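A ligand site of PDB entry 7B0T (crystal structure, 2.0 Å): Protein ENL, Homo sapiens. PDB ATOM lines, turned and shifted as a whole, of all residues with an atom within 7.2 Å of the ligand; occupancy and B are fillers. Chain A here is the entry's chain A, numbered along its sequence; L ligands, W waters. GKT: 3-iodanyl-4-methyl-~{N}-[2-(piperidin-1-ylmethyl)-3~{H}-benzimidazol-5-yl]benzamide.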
ATOM      1  N   GLU A  26      29.306 -11.346 -15.178  1.00  0.00           N
ATOM      2  CA  GLU A  26      29.350 -12.737 -14.625  1.00  0.00           C
ATOM      3  C   GLU A  26      28.081 -13.516 -14.971  1.00  0.00           C
ATOM      4  O   GLU A  26      27.899 -14.580 -14.358  1.00  0.00           O
ATOM      5  CB  GLU A  26      29.506 -12.745 -13.108  1.00  0.00           C
ATOM      6  CG  GLU A  26      30.447 -11.681 -12.582  1.00  0.00           C
ATOM      7  CD  GLU A  26      29.733 -10.607 -11.790  1.00  0.00           C
ATOM      8  OE1 GLU A  26      28.922  -9.871 -12.406  1.00  0.00           O
ATOM      9  OE2 GLU A  26      29.931 -10.545 -10.556  1.00  0.00           O
ATOM     10  N   PHE A  28      24.826 -12.922 -14.345  1.00  0.00           N
ATOM     11  CA  PHE A  28      23.601 -12.706 -13.515  1.00  0.00           C
ATOM     12  C   PHE A  28      22.601 -11.888 -14.325  1.00  0.00           C
ATOM     13  O   PHE A  28      22.928 -10.796 -14.825  1.00  0.00           O
ATOM     14  CB  PHE A  28      23.941 -12.017 -12.184  1.00  0.00           C
ATOM     15  CG  PHE A  28      25.039 -12.707 -11.413  1.00  0.00           C
ATOM     16  CD1 PHE A  28      25.052 -14.082 -11.265  1.00  0.00           C
ATOM     17  CD2 PHE A  28      26.074 -11.970 -10.869  1.00  0.00           C
ATOM     18  CE1 PHE A  28      26.078 -14.718 -10.576  1.00  0.00           C
ATOM     19  CE2 PHE A  28      27.100 -12.606 -10.180  1.00  0.00           C
ATOM     20  CZ  PHE A  28      27.111 -13.973 -10.047  1.00  0.00           C
ATOM     21  N   HIS A  30      19.419 -11.199 -13.133  1.00  0.00           N
ATOM     22  CA  HIS A  30      18.378 -10.696 -12.204  1.00  0.00           C
ATOM     23  C   HIS A  30      18.997 -10.127 -10.927  1.00  0.00           C
ATOM     24  O   HIS A  30      19.967 -10.723 -10.388  1.00  0.00           O
ATOM     25  CB  HIS A  30      17.374 -11.796 -11.874  1.00  0.00           C
ATOM     26  CG  HIS A  30      16.393 -12.113 -12.959  1.00  0.00           C
ATOM     27  ND1 HIS A  30      16.710 -12.939 -14.019  1.00  0.00           N
ATOM     28  CD2 HIS A  30      15.065 -11.836 -13.055  1.00  0.00           C
ATOM     29  CE1 HIS A  30      15.619 -13.125 -14.753  1.00  0.00           C
ATOM     30  NE2 HIS A  30      14.596 -12.455 -14.183  1.00  0.00           N
ATOM     31  N   TRP A  32      17.602  -9.354  -7.093  1.00  0.00           N
ATOM     32  CA  TRP A  32      16.465  -9.631  -6.190  1.00  0.00           C
ATOM     33  C   TRP A  32      16.801  -9.195  -4.766  1.00  0.00           C
ATOM     34  O   TRP A  32      18.004  -8.981  -4.417  1.00  0.00           O
ATOM     35  CB  TRP A  32      16.038 -11.107  -6.284  1.00  0.00           C
ATOM     36  CG  TRP A  32      17.096 -12.139  -6.025  1.00  0.00           C
ATOM     37  CD1 TRP A  32      17.724 -12.926  -6.949  1.00  0.00           C
ATOM     38  CD2 TRP A  32      17.545 -12.618  -4.740  1.00  0.00           C
ATOM     39  NE1 TRP A  32      18.577 -13.795  -6.330  1.00  0.00           N
ATOM     40  CE2 TRP A  32      18.473 -13.649  -4.975  1.00  0.00           C
ATOM     41  CE3 TRP A  32      17.245 -12.271  -3.414  1.00  0.00           C
ATOM     42  CZ2 TRP A  32      19.104 -14.332  -3.943  1.00  0.00           C
ATOM     43  CZ3 TRP A  32      17.895 -12.928  -2.390  1.00  0.00           C
ATOM     44  CH2 TRP A  32      18.812 -13.942  -2.661  1.00  0.00           C
ATOM     45  N   LEU A  55      20.217 -19.394   1.283  1.00  0.00           N
ATOM     46  CA  LEU A  55      20.277 -19.164  -0.181  1.00  0.00           C
ATOM     47  C   LEU A  55      20.655 -20.473  -0.876  1.00  0.00           C
ATOM     48  O   LEU A  55      21.205 -21.352  -0.207  1.00  0.00           O
ATOM     49  CB  LEU A  55      21.324 -18.077  -0.470  1.00  0.00           C
ATOM     50  CG  LEU A  55      20.797 -16.643  -0.484  1.00  0.00           C
ATOM     51  CD1 LEU A  55      20.099 -16.309   0.814  1.00  0.00           C
ATOM     52  CD2 LEU A  55      21.924 -15.652  -0.747  1.00  0.00           C
ATOM     53  N   HIS A  56      20.425 -20.570  -2.179  1.00  0.00           N
ATOM     54  CA  HIS A  56      20.868 -21.720  -3.025  1.00  0.00           C
ATOM     55  C   HIS A  56      22.347 -21.979  -2.749  1.00  0.00           C
ATOM     56  O   HIS A  56      23.077 -20.974  -2.485  1.00  0.00           O
ATOM     57  CB  HIS A  56      20.585 -21.450  -4.499  1.00  0.00           C
ATOM     58  CG  HIS A  56      20.896 -22.627  -5.367  1.00  0.00           C
ATOM     59  ND1 HIS A  56      19.989 -23.629  -5.593  1.00  0.00           N
ATOM     60  CD2 HIS A  56      22.030 -23.004  -5.966  1.00  0.00           C
ATOM     61  CE1 HIS A  56      20.527 -24.546  -6.341  1.00  0.00           C
ATOM     62  NE2 HIS A  56      21.783 -24.181  -6.601  1.00  0.00           N
ATOM     63  N   ASP A  57      22.785 -23.260  -2.736  1.00  0.00           N
ATOM     64  CA  ASP A  57      24.129 -23.689  -2.217  1.00  0.00           C
ATOM     65  C   ASP A  57      25.223 -23.147  -3.136  1.00  0.00           C
ATOM     66  O   ASP A  57      26.374 -23.065  -2.709  1.00  0.00           O
ATOM     67  CB  ASP A  57      24.231 -25.209  -2.011  1.00  0.00           C
ATOM     68  CG  ASP A  57      23.686 -25.708  -0.672  1.00  0.00           C
ATOM     69  OD1 ASP A  57      23.509 -24.886   0.220  1.00  0.00           O
ATOM     70  OD2 ASP A  57      23.425 -26.905  -0.545  1.00  0.00           O
ATOM     71  N   SER A  58      24.848 -22.668  -4.330  1.00  0.00           N
ATOM     72  CA  SER A  58      25.747 -22.034  -5.319  1.00  0.00           C
ATOM     73  C   SER A  58      26.240 -20.672  -4.819  1.00  0.00           C
ATOM     74  O   SER A  58      27.283 -20.258  -5.242  1.00  0.00           O
ATOM     75  CB  SER A  58      25.081 -21.921  -6.664  1.00  0.00           C
ATOM     76  OG  SER A  58      24.035 -20.973  -6.654  1.00  0.00           O
ATOM     77  N   PHE A  59      25.472 -19.974  -3.988  1.00  0.00           N
ATOM     78  CA  PHE A  59      25.820 -18.619  -3.464  1.00  0.00           C
ATOM     79  C   PHE A  59      26.961 -18.722  -2.464  1.00  0.00           C
ATOM     80  O   PHE A  59      27.004 -19.671  -1.678  1.00  0.00           O
ATOM     81  CB  PHE A  59      24.624 -17.962  -2.753  1.00  0.00           C
ATOM     82  CG  PHE A  59      23.593 -17.351  -3.666  1.00  0.00           C
ATOM     83  CD1 PHE A  59      22.542 -18.090  -4.183  1.00  0.00           C
ATOM     84  CD2 PHE A  59      23.677 -16.010  -4.034  1.00  0.00           C
ATOM     85  CE1 PHE A  59      21.605 -17.519  -5.028  1.00  0.00           C
ATOM     86  CE2 PHE A  59      22.741 -15.439  -4.879  1.00  0.00           C
ATOM     87  CZ  PHE A  59      21.711 -16.201  -5.377  1.00  0.00           C
ATOM     88  N   PRO A  60      27.886 -17.743  -2.424  1.00  0.00           N
ATOM     89  CA  PRO A  60      28.886 -17.692  -1.359  1.00  0.00           C
ATOM     90  C   PRO A  60      28.204 -17.355  -0.028  1.00  0.00           C
ATOM     91  O   PRO A  60      27.224 -16.645  -0.055  1.00  0.00           O
ATOM     92  CB  PRO A  60      29.885 -16.611  -1.819  1.00  0.00           C
ATOM     93  CG  PRO A  60      29.123 -15.788  -2.860  1.00  0.00           C
ATOM     94  CD  PRO A  60      28.071 -16.703  -3.447  1.00  0.00           C
ATOM     95  N   LYS A  61      28.629 -18.008   1.053  1.00  0.00           N
ATOM     96  CA  LYS A  61      28.036 -17.882   2.412  1.00  0.00           C
ATOM     97  C   LYS A  61      26.506 -17.917   2.298  1.00  0.00           C
ATOM     98  O   LYS A  61      25.839 -16.898   2.547  1.00  0.00           O
ATOM     99  CB  LYS A  61      28.492 -16.580   3.075  1.00  0.00           C
ATOM    100  CG  LYS A  61      29.961 -16.220   2.871  1.00  0.00           C
ATOM    101  CD  LYS A  61      30.900 -16.790   3.920  1.00  0.00           C
ATOM    102  CE  LYS A  61      32.330 -16.301   3.763  1.00  0.00           C
ATOM    103  NZ  LYS A  61      32.478 -14.878   4.127  1.00  0.00           N
ATOM    104  N   ARG A  64      22.818 -16.609   5.274  1.00  0.00           N
ATOM    105  CA  ARG A  64      22.846 -15.155   5.474  1.00  0.00           C
ATOM    106  C   ARG A  64      21.965 -14.816   6.687  1.00  0.00           C
ATOM    107  O   ARG A  64      20.791 -15.178   6.684  1.00  0.00           O
ATOM    108  CB  ARG A  64      22.396 -14.411   4.221  1.00  0.00           C
ATOM    109  CG  ARG A  64      23.120 -14.810   2.944  1.00  0.00           C
ATOM    110  CD  ARG A  64      24.498 -14.223   2.813  1.00  0.00           C
ATOM    111  NE  ARG A  64      25.028 -14.573   1.515  1.00  0.00           N
ATOM    112  CZ  ARG A  64      24.827 -13.891   0.402  1.00  0.00           C
ATOM    113  NH1 ARG A  64      25.308 -14.341  -0.740  1.00  0.00           N
ATOM    114  NH2 ARG A  64      24.110 -12.773   0.427  1.00  0.00           N
ATOM    115  N   GLU A  74      20.040  -8.713  -0.354  1.00  0.00           N
ATOM    116  CA  GLU A  74      20.037  -8.156  -1.733  1.00  0.00           C
ATOM    117  C   GLU A  74      21.061  -8.957  -2.539  1.00  0.00           C
ATOM    118  O   GLU A  74      22.206  -9.089  -2.102  1.00  0.00           O
ATOM    119  CB  GLU A  74      20.339  -6.660  -1.682  1.00  0.00           C
ATOM    120  CG  GLU A  74      19.104  -5.768  -1.815  1.00  0.00           C
ATOM    121  CD  GLU A  74      19.155  -4.420  -1.081  1.00  0.00           C
ATOM    122  OE1 GLU A  74      20.152  -4.149  -0.391  1.00  0.00           O
ATOM    123  OE2 GLU A  74      18.179  -3.641  -1.196  1.00  0.00           O
ATOM    124  N   GLU A  75      20.651  -9.543  -3.641  1.00  0.00           N
ATOM    125  CA  GLU A  75      21.597 -10.346  -4.433  1.00  0.00           C
ATOM    126  C   GLU A  75      21.338 -10.132  -5.901  1.00  0.00           C
ATOM    127  O   GLU A  75      20.317  -9.570  -6.268  1.00  0.00           O
ATOM    128  CB  GLU A  75      21.475 -11.834  -4.070  1.00  0.00           C
ATOM    129  CG  GLU A  75      22.463 -12.269  -3.017  1.00  0.00           C
ATOM    130  CD  GLU A  75      23.893 -12.265  -3.491  1.00  0.00           C
ATOM    131  OE1 GLU A  75      24.113 -11.957  -4.703  1.00  0.00           O
ATOM    132  OE2 GLU A  75      24.781 -12.582  -2.674  1.00  0.00           O
ATOM    133  N   SER A  76      22.231 -10.643  -6.688  1.00  0.00           N
ATOM    134  CA  SER A  76      21.961 -10.946  -8.099  1.00  0.00           C
ATOM    135  C   SER A  76      22.090 -12.463  -8.296  1.00  0.00           C
ATOM    136  O   SER A  76      22.685 -13.143  -7.418  1.00  0.00           O
ATOM    137  CB  SER A  76      22.883 -10.143  -8.979  1.00  0.00           C
ATOM    138  OG  SER A  76      22.421  -8.806  -9.058  1.00  0.00           O
ATOM    139  N   GLY A  77      21.475 -12.979  -9.361  1.00  0.00           N
ATOM    140  CA  GLY A  77      21.525 -14.409  -9.701  1.00  0.00           C
ATOM    141  C   GLY A  77      20.916 -14.661 -11.051  1.00  0.00           C
ATOM    142  O   GLY A  77      20.623 -13.690 -11.775  1.00  0.00           O
ATOM    143  N   TYR A  78      20.735 -15.921 -11.409  1.00  0.00           N
ATOM    144  CA  TYR A  78      20.279 -16.292 -12.779  1.00  0.00           C
ATOM    145  C   TYR A  78      19.015 -17.153 -12.729  1.00  0.00           C
ATOM    146  O   TYR A  78      18.391 -17.280 -13.765  1.00  0.00           O
ATOM    147  CB  TYR A  78      21.424 -16.920 -13.575  1.00  0.00           C
ATOM    148  CG  TYR A  78      22.458 -17.662 -12.766  1.00  0.00           C
ATOM    149  CD1 TYR A  78      23.733 -17.171 -12.597  1.00  0.00           C
ATOM    150  CD2 TYR A  78      22.182 -18.923 -12.284  1.00  0.00           C
ATOM    151  CE1 TYR A  78      24.697 -17.885 -11.898  1.00  0.00           C
ATOM    152  CE2 TYR A  78      23.138 -19.658 -11.595  1.00  0.00           C
ATOM    153  CZ  TYR A  78      24.392 -19.135 -11.387  1.00  0.00           C
ATOM    154  OH  TYR A  78      25.320 -19.890 -10.734  1.00  0.00           O
ATOM    155  N   ALA A  79      18.579 -17.616 -11.540  1.00  0.00           N
ATOM    156  CA  ALA A  79      17.413 -18.513 -11.386  1.00  0.00           C
ATOM    157  C   ALA A  79      16.729 -18.266 -10.031  1.00  0.00           C
ATOM    158  O   ALA A  79      17.413 -17.824  -9.072  1.00  0.00           O
ATOM    159  CB  ALA A  79      17.863 -19.943 -11.514  1.00  0.00           C
ATOM    160  N   GLY A  80      15.439 -18.569  -9.952  1.00  0.00           N
ATOM    161  CA  GLY A  80      14.684 -18.664  -8.696  1.00  0.00           C
ATOM    162  C   GLY A  80      15.072 -19.931  -7.952  1.00  0.00           C
ATOM    163  O   GLY A  80      15.745 -20.771  -8.560  1.00  0.00           O
ATOM    164  N   PHE A  81      14.703 -20.053  -6.677  1.00  0.00           N
ATOM    165  CA  PHE A  81      14.886 -21.290  -5.882  1.00  0.00           C
ATOM    166  C   PHE A  81      14.008 -21.206  -4.643  1.00  0.00           C
ATOM    167  O   PHE A  81      13.400 -20.149  -4.406  1.00  0.00           O
ATOM    168  CB  PHE A  81      16.353 -21.475  -5.479  1.00  0.00           C
ATOM    169  CG  PHE A  81      16.969 -20.262  -4.841  1.00  0.00           C
ATOM    170  CD1 PHE A  81      17.376 -19.198  -5.608  1.00  0.00           C
ATOM    171  CD2 PHE A  81      17.076 -20.167  -3.454  1.00  0.00           C
ATOM    172  CE1 PHE A  81      17.899 -18.054  -5.004  1.00  0.00           C
ATOM    173  CE2 PHE A  81      17.588 -19.031  -2.854  1.00  0.00           C
ATOM    174  CZ  PHE A  81      18.014 -17.973  -3.633  1.00  0.00           C
ATOM    175  N   LEU A 104      11.404 -18.065  -3.784  1.00  0.00           N
ATOM    176  CA  LEU A 104      12.078 -16.927  -4.452  1.00  0.00           C
ATOM    177  C   LEU A 104      12.028 -17.136  -5.952  1.00  0.00           C
ATOM    178  O   LEU A 104      13.026 -17.582  -6.516  1.00  0.00           O
ATOM    179  CB  LEU A 104      13.526 -16.825  -4.023  1.00  0.00           C
ATOM    180  CG  LEU A 104      14.114 -15.489  -4.403  1.00  0.00           C
ATOM    181  CD1 LEU A 104      13.898 -14.467  -3.279  1.00  0.00           C
ATOM    182  CD2 LEU A 104      15.551 -15.623  -4.761  1.00  0.00           C
ATOM    183  N   LEU A 106      11.534 -15.797  -9.958  1.00  0.00           N
ATOM    184  CA  LEU A 106      11.925 -14.665 -10.838  1.00  0.00           C
ATOM    185  C   LEU A 106      10.896 -14.564 -11.963  1.00  0.00           C
ATOM    186  O   LEU A 106      10.315 -15.605 -12.320  1.00  0.00           O
ATOM    187  CB  LEU A 106      13.308 -14.927 -11.418  1.00  0.00           C
ATOM    188  CG  LEU A 106      14.450 -15.091 -10.412  1.00  0.00           C
ATOM    189  CD1 LEU A 106      15.778 -15.200 -11.141  1.00  0.00           C
ATOM    190  CD2 LEU A 106      14.489 -13.939  -9.427  1.00  0.00           C
HETATM  191  C1  GKT L   1      19.898 -22.034  -9.135  1.00  0.00           C
HETATM  192  C2  GKT L   1      19.360 -20.830  -8.660  1.00  0.00           C
HETATM  193  C3  GKT L   1      20.160 -19.726  -8.395  1.00  0.00           C
HETATM  194  C4  GKT L   1      21.538 -19.787  -8.569  1.00  0.00           C
HETATM  195  C5  GKT L   1      22.104 -20.989  -8.993  1.00  0.00           C
HETATM  196  C6  GKT L   1      21.307 -22.082  -9.319  1.00  0.00           C
HETATM  197  C7  GKT L   1      22.337 -18.530  -8.445  1.00  0.00           C
HETATM  198  O   GKT L   1      21.923 -17.476  -8.940  1.00  0.00           O
HETATM  199  I   GKT L   1      22.147 -23.771 -10.292  1.00  0.00           I
HETATM  200  C   GKT L   1      18.991 -23.195  -9.447  1.00  0.00           C
HETATM  201  N   GKT L   1      23.514 -18.644  -7.790  1.00  0.00           N
HETATM  202  C8  GKT L   1      24.506 -17.642  -7.587  1.00  0.00           C
HETATM  203  C20 GKT L   1      24.207 -16.278  -7.601  1.00  0.00           C
HETATM  204  C19 GKT L   1      25.190 -15.368  -7.209  1.00  0.00           C
HETATM  205  C11 GKT L   1      26.454 -15.835  -6.834  1.00  0.00           C
HETATM  206  C10 GKT L   1      26.762 -17.187  -6.853  1.00  0.00           C
HETATM  207  C9  GKT L   1      25.790 -18.087  -7.241  1.00  0.00           C
HETATM  208  N3  GKT L   1      25.168 -13.975  -7.129  1.00  0.00           N
HETATM  209  C12 GKT L   1      26.383 -13.632  -6.738  1.00  0.00           C
HETATM  210  N1  GKT L   1      27.196 -14.702  -6.528  1.00  0.00           N
HETATM  211  C13 GKT L   1      26.911 -12.224  -6.743  1.00  0.00           C
HETATM  212  N2  GKT L   1      27.510 -11.787  -5.475  1.00  0.00           N
HETATM  213  C18 GKT L   1      26.961 -10.494  -5.043  1.00  0.00           C
HETATM  214  C17 GKT L   1      27.697  -9.952  -3.844  1.00  0.00           C
HETATM  215  C16 GKT L   1      27.649 -10.926  -2.687  1.00  0.00           C
HETATM  216  C15 GKT L   1      28.105 -12.313  -3.122  1.00  0.00           C
HETATM  217  C14 GKT L   1      27.361 -12.771  -4.387  1.00  0.00           C
HETATM  218  O   HOH W   1      19.373 -16.180  -7.836  1.00  0.00           O
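The side-chain carboxylate (OE1) of Glu 75 lies within salt-bridge range of a nitrogen (N2) of the ligand. The backbone carbonyl oxygen (O) of Ser 76 is in hydrogen-bond range of a nitrogen (N3) of the ligand (2.6 Å). N of Tyr 78 is in hydrogen-bond range of O of the ligand, at 3.2 Å. The side-chain hydroxyl of Ser 58 is in hydrogen-bond range of a nitrogen (N) of the ligand, at 2.6 Å.
The side-chain hydroxyl (OG) of Ser 76 lies close to the backbone carbonyl oxygen (O) of His 30. N of Glu 75 sits at hydrogen-bond distance from O of Trp 32 (2.8 Å). The guanidinium group of Arg 64 lies within salt-bridge range of the side-chain carboxylate of Glu 75. O of His 30 is in hydrogen-bond range of N of Gly 77 (2.9 Å). The backbone carbonyl oxygen (O) of Phe 81 is in hydrogen-bond range of the backbone NH (N) of Leu 104. NH1 of Arg 64 lies within hydrogen-bond range of O of Pro 60, 3.1 Å away.
Residues that only touch the ligand: Gly 77, Phe 59, Ala 79, Phe 28, His 56, Gly 80, Pro 60 and Phe 81. Within 4 Å of the ligand: Phe 28, His 56, Ser 58, Phe 59, Pro 60, Glu 75, Ser 76, Gly 77, Tyr 78, Ala 79, Gly 80 and Phe 81. The nearest printed residue that does not touch the ligand is Arg 64 (4.2 Å).
Water W1 lies within hydrogen-bond range of O of Ala 79 (2.8 Å), NE1 of Trp 32 (2.9 Å) and O of the ligand (3.1 Å).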
